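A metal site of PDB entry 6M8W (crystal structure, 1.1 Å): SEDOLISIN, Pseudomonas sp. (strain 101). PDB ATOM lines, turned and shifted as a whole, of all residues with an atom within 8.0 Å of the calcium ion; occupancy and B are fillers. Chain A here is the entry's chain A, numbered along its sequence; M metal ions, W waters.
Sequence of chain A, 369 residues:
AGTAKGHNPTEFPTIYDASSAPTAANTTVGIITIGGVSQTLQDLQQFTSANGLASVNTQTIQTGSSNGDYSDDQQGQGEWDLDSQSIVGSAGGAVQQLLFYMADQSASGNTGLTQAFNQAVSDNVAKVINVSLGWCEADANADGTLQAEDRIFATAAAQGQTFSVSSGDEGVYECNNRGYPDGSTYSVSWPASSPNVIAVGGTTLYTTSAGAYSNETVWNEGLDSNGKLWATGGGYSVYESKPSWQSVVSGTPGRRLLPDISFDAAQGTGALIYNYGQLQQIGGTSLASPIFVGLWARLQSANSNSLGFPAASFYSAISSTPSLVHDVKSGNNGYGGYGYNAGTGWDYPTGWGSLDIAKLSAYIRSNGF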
ATOM      1  N   VAL A 218     -22.430  11.377   1.597  1.00  0.00           N
ATOM      2  CA  VAL A 218     -22.218  11.884   2.934  1.00  0.00           C
ATOM      3  C   VAL A 218     -22.810  13.278   3.048  1.00  0.00           C
ATOM      4  O   VAL A 218     -22.718  14.071   2.112  1.00  0.00           O
ATOM      5  CB  VAL A 218     -20.707  11.942   3.233  1.00  0.00           C
ATOM      6  CG1 VAL A 218     -20.416  12.583   4.583  1.00  0.00           C
ATOM      7  CG2 VAL A 218     -20.103  10.525   3.175  1.00  0.00           C
ATOM      8  N   VAL A 325     -29.532  -2.347   3.185  1.00  0.00           N
ATOM      9  CA  VAL A 325     -29.151  -0.944   3.303  1.00  0.00           C
ATOM     10  C   VAL A 325     -28.872  -0.323   1.947  1.00  0.00           C
ATOM     11  O   VAL A 325     -28.523  -0.998   0.969  1.00  0.00           O
ATOM     12  CB  VAL A 325     -27.943  -0.719   4.231  1.00  0.00           C
ATOM     13  CG1 VAL A 325     -28.307  -1.085   5.669  1.00  0.00           C
ATOM     14  CG2 VAL A 325     -26.692  -1.448   3.740  1.00  0.00           C
ATOM     15  N   HIS A 326     -28.932   1.013   1.948  1.00  0.00           N
ATOM     16  CA  HIS A 326     -28.334   1.844   0.918  1.00  0.00           C
ATOM     17  C   HIS A 326     -26.937   2.218   1.430  1.00  0.00           C
ATOM     18  O   HIS A 326     -26.826   3.004   2.354  1.00  0.00           O
ATOM     19  CB  HIS A 326     -29.116   3.119   0.651  1.00  0.00           C
ATOM     20  CG  HIS A 326     -30.495   2.879   0.173  1.00  0.00           C
ATOM     21  ND1 HIS A 326     -30.787   2.366  -1.064  1.00  0.00           N
ATOM     22  CD2 HIS A 326     -31.704   3.081   0.742  1.00  0.00           C
ATOM     23  CE1 HIS A 326     -32.087   2.269  -1.269  1.00  0.00           C
ATOM     24  NE2 HIS A 326     -32.698   2.689  -0.163  1.00  0.00           N
ATOM     25  N   ASP A 327     -25.918   1.613   0.827  1.00  0.00           N
ATOM     26  CA  ASP A 327     -24.538   1.798   1.239  1.00  0.00           C
ATOM     27  C   ASP A 327     -24.025   3.131   0.687  1.00  0.00           C
ATOM     28  O   ASP A 327     -23.875   3.276  -0.513  1.00  0.00           O
ATOM     29  CB  ASP A 327     -23.697   0.625   0.736  1.00  0.00           C
ATOM     30  CG  ASP A 327     -22.251   0.708   1.148  1.00  0.00           C
ATOM     31  OD1 ASP A 327     -21.927   1.463   2.103  1.00  0.00           O
ATOM     32  OD2 ASP A 327     -21.446  -0.004   0.506  1.00  0.00           O
ATOM     33  N   VAL A 328     -23.744   4.091   1.528  1.00  0.00           N
ATOM     34  CA  VAL A 328     -23.172   5.372   1.096  1.00  0.00           C
ATOM     35  C   VAL A 328     -21.713   5.137   0.781  1.00  0.00           C
ATOM     36  O   VAL A 328     -20.994   4.544   1.589  1.00  0.00           O
ATOM     37  CB  VAL A 328     -23.382   6.436   2.184  1.00  0.00           C
ATOM     38  CG1 VAL A 328     -22.691   7.723   1.758  1.00  0.00           C
ATOM     39  CG2 VAL A 328     -24.868   6.606   2.441  1.00  0.00           C
ATOM     40  N   LYS A 329     -21.261   5.623  -0.371  1.00  0.00           N
ATOM     41  CA  LYS A 329     -19.909   5.396  -0.842  1.00  0.00           C
ATOM     42  C   LYS A 329     -19.120   6.665  -1.122  1.00  0.00           C
ATOM     43  O   LYS A 329     -17.874   6.583  -1.228  1.00  0.00           O
ATOM     44  CB  LYS A 329     -19.891   4.500  -2.079  1.00  0.00           C
ATOM     45  CG  LYS A 329     -20.362   3.085  -1.762  1.00  0.00           C
ATOM     46  CD  LYS A 329     -20.519   2.297  -3.080  1.00  0.00           C
ATOM     47  CE  LYS A 329     -20.989   0.893  -2.868  1.00  0.00           C
ATOM     48  NZ  LYS A 329     -20.750   0.084  -4.106  1.00  0.00           N
ATOM     49  N   SER A 330     -19.787   7.824  -1.259  1.00  0.00           N
ATOM     50  CA  SER A 330     -19.099   9.041  -1.700  1.00  0.00           C
ATOM     51  C   SER A 330     -19.213  10.142  -0.657  1.00  0.00           C
ATOM     52  O   SER A 330     -20.310  10.413  -0.153  1.00  0.00           O
ATOM     53  CB  SER A 330     -19.707   9.523  -3.019  1.00  0.00           C
ATOM     54  OG  SER A 330     -19.246  10.807  -3.415  1.00  0.00           O
ATOM     55  N   ASN A 341     -13.579   9.297   5.075  1.00  0.00           N
ATOM     56  CA  ASN A 341     -14.209   9.127   3.765  1.00  0.00           C
ATOM     57  C   ASN A 341     -15.205   7.980   3.817  1.00  0.00           C
ATOM     58  O   ASN A 341     -14.965   6.955   4.445  1.00  0.00           O
ATOM     59  CB  ASN A 341     -13.156   8.792   2.714  1.00  0.00           C
ATOM     60  CG  ASN A 341     -12.145   9.900   2.627  1.00  0.00           C
ATOM     61  OD1 ASN A 341     -12.504  11.054   2.334  1.00  0.00           O
ATOM     62  ND2 ASN A 341     -10.884   9.604   2.891  1.00  0.00           N
ATOM     63  N   ALA A 342     -16.311   8.145   3.110  1.00  0.00           N
ATOM     64  CA  ALA A 342     -17.210   7.025   2.900  1.00  0.00           C
ATOM     65  C   ALA A 342     -16.548   5.987   2.001  1.00  0.00           C
ATOM     66  O   ALA A 342     -15.579   6.263   1.279  1.00  0.00           O
ATOM     67  CB  ALA A 342     -18.531   7.477   2.270  1.00  0.00           C
ATOM     68  N   GLY A 343     -17.071   4.787   2.058  1.00  0.00           N
ATOM     69  CA  GLY A 343     -16.523   3.730   1.236  1.00  0.00           C
ATOM     70  C   GLY A 343     -17.457   2.533   1.257  1.00  0.00           C
ATOM     71  O   GLY A 343     -18.589   2.596   1.782  1.00  0.00           O
ATOM     72  N   THR A 344     -16.994   1.419   0.665  1.00  0.00           N
ATOM     73  CA  THR A 344     -17.802   0.219   0.623  1.00  0.00           C
ATOM     74  C   THR A 344     -18.085  -0.288   2.026  1.00  0.00           C
ATOM     75  O   THR A 344     -17.159  -0.397   2.826  1.00  0.00           O
ATOM     76  CB  THR A 344     -17.047  -0.857  -0.175  1.00  0.00           C
ATOM     77  OG1 THR A 344     -16.914  -0.342  -1.517  1.00  0.00           O
ATOM     78  CG2 THR A 344     -17.814  -2.170  -0.201  1.00  0.00           C
ATOM     79  N   GLY A 345     -19.334  -0.623   2.344  1.00  0.00           N
ATOM     80  CA  GLY A 345     -19.720  -1.149   3.616  1.00  0.00           C
ATOM     81  C   GLY A 345     -19.681  -0.111   4.714  1.00  0.00           C
ATOM     82  O   GLY A 345     -19.883   1.101   4.468  1.00  0.00           O
ATOM     83  N   TRP A 346     -19.452  -0.517   5.959  1.00  0.00           N
ATOM     84  CA  TRP A 346     -19.487   0.383   7.096  1.00  0.00           C
ATOM     85  C   TRP A 346     -18.398   1.442   6.951  1.00  0.00           C
ATOM     86  O   TRP A 346     -17.246   1.077   6.667  1.00  0.00           O
ATOM     87  CB  TRP A 346     -19.335  -0.418   8.379  1.00  0.00           C
ATOM     88  CG  TRP A 346     -19.662   0.423   9.610  1.00  0.00           C
ATOM     89  CD1 TRP A 346     -20.841   0.403  10.305  1.00  0.00           C
ATOM     90  CD2 TRP A 346     -18.828   1.381  10.279  1.00  0.00           C
ATOM     91  NE1 TRP A 346     -20.771   1.272  11.346  1.00  0.00           N
ATOM     92  CE2 TRP A 346     -19.559   1.910  11.351  1.00  0.00           C
ATOM     93  CE3 TRP A 346     -17.515   1.863  10.100  1.00  0.00           C
ATOM     94  CZ2 TRP A 346     -19.035   2.889  12.191  1.00  0.00           C
ATOM     95  CZ3 TRP A 346     -17.010   2.828  10.933  1.00  0.00           C
ATOM     96  CH2 TRP A 346     -17.786   3.334  11.972  1.00  0.00           C
ATOM     97  N   ASP A 347     -18.709   2.717   7.162  1.00  0.00           N
ATOM     98  CA  ASP A 347     -17.686   3.758   7.164  1.00  0.00           C
ATOM     99  C   ASP A 347     -17.954   4.740   8.298  1.00  0.00           C
ATOM    100  O   ASP A 347     -19.053   4.774   8.913  1.00  0.00           O
ATOM    101  CB  ASP A 347     -17.551   4.387   5.804  1.00  0.00           C
ATOM    102  CG  ASP A 347     -18.861   4.984   5.276  1.00  0.00           C
ATOM    103  OD1 ASP A 347     -19.453   5.834   5.994  1.00  0.00           O
ATOM    104  OD2 ASP A 347     -19.241   4.564   4.153  1.00  0.00           O
ATOM    105  N   TYR A 348     -16.954   5.558   8.636  1.00  0.00           N
ATOM    106  CA  TYR A 348     -17.104   6.466   9.758  1.00  0.00           C
ATOM    107  C   TYR A 348     -18.091   7.605   9.487  1.00  0.00           C
ATOM    108  O   TYR A 348     -18.741   8.035  10.457  1.00  0.00           O
ATOM    109  CB  TYR A 348     -15.734   7.005  10.163  1.00  0.00           C
ATOM    110  CG  TYR A 348     -14.874   6.005  10.871  1.00  0.00           C
ATOM    111  CD1 TYR A 348     -15.181   5.620  12.168  1.00  0.00           C
ATOM    112  CD2 TYR A 348     -13.757   5.418  10.293  1.00  0.00           C
ATOM    113  CE1 TYR A 348     -14.424   4.709  12.886  1.00  0.00           C
ATOM    114  CE2 TYR A 348     -12.989   4.502  10.964  1.00  0.00           C
ATOM    115  CZ  TYR A 348     -13.333   4.145  12.279  1.00  0.00           C
ATOM    116  OH  TYR A 348     -12.582   3.230  13.009  1.00  0.00           O
ATOM    117  N   PRO A 349     -18.250   8.150   8.269  1.00  0.00           N
ATOM    118  CA  PRO A 349     -19.246   9.208   8.155  1.00  0.00           C
ATOM    119  C   PRO A 349     -20.682   8.745   8.346  1.00  0.00           C
ATOM    120  O   PRO A 349     -21.517   9.502   8.846  1.00  0.00           O
ATOM    121  CB  PRO A 349     -18.981   9.773   6.759  1.00  0.00           C
ATOM    122  CG  PRO A 349     -17.514   9.530   6.547  1.00  0.00           C
ATOM    123  CD  PRO A 349     -17.346   8.110   7.104  1.00  0.00           C
ATOM    124  N   THR A 350     -20.997   7.526   7.880  1.00  0.00           N
ATOM    125  CA  THR A 350     -22.369   7.120   7.719  1.00  0.00           C
ATOM    126  C   THR A 350     -22.689   5.759   8.310  1.00  0.00           C
ATOM    127  O   THR A 350     -23.885   5.325   8.246  1.00  0.00           O
ATOM    128  CB  THR A 350     -22.826   7.142   6.232  1.00  0.00           C
ATOM    129  OG1 THR A 350     -22.071   6.220   5.423  1.00  0.00           O
ATOM    130  CG2 THR A 350     -22.753   8.550   5.668  1.00  0.00           C
ATOM    131  N   GLY A 351     -21.746   5.057   8.881  1.00  0.00           N
ATOM    132  CA  GLY A 351     -22.015   3.711   9.394  1.00  0.00           C
ATOM    133  C   GLY A 351     -22.432   2.794   8.252  1.00  0.00           C
ATOM    134  O   GLY A 351     -21.787   2.791   7.180  1.00  0.00           O
ATOM    135  N   TRP A 352     -23.502   2.008   8.437  1.00  0.00           N
ATOM    136  CA  TRP A 352     -23.969   1.124   7.395  1.00  0.00           C
ATOM    137  C   TRP A 352     -24.742   1.845   6.288  1.00  0.00           C
ATOM    138  O   TRP A 352     -25.070   1.174   5.298  1.00  0.00           O
ATOM    139  CB  TRP A 352     -24.851   0.042   8.014  1.00  0.00           C
ATOM    140  CG  TRP A 352     -24.150  -0.946   8.874  1.00  0.00           C
ATOM    141  CD1 TRP A 352     -24.300  -1.112  10.219  1.00  0.00           C
ATOM    142  CD2 TRP A 352     -23.182  -1.909   8.459  1.00  0.00           C
ATOM    143  NE1 TRP A 352     -23.513  -2.129  10.668  1.00  0.00           N
ATOM    144  CE2 TRP A 352     -22.798  -2.640   9.595  1.00  0.00           C
ATOM    145  CE3 TRP A 352     -22.596  -2.262   7.214  1.00  0.00           C
ATOM    146  CZ2 TRP A 352     -21.840  -3.681   9.543  1.00  0.00           C
ATOM    147  CZ3 TRP A 352     -21.666  -3.272   7.178  1.00  0.00           C
ATOM    148  CH2 TRP A 352     -21.286  -3.977   8.332  1.00  0.00           C
ATOM    149  N   GLY A 353     -25.062   3.102   6.444  1.00  0.00           N
ATOM    150  CA  GLY A 353     -25.933   3.799   5.515  1.00  0.00           C
ATOM    151  C   GLY A 353     -27.373   3.752   5.967  1.00  0.00           C
ATOM    152  O   GLY A 353     -27.631   3.577   7.175  1.00  0.00           O
HETATM  153 CA    CA M   1     -20.451   2.912   3.116  1.00  0.00          CA
HETATM  154  O   HOH W   1     -22.272   3.582   4.555  1.00  0.00           O
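OD1 of Asp 347 sits at hydrogen-bond distance from OG1 of Thr 350.
The nearest printed residue that does not touch the calcium ion is Thr 344 (4.1 Å).
The calcium ion is bound by the side-chain carboxylate (OD2) of Asp 347, the backbone carbonyl oxygen (O) of Val 328, the side-chain carboxylate (OD1) of Asp 327, the backbone carbonyl oxygen (O) of Gly 343, the backbone carbonyl oxygen (O) of Gly 345 and water W1.
Water W1 lies within hydrogen-bond range of OG1 of Thr 350, O of Gly 351, N of Gly 353 and N of Val 328.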
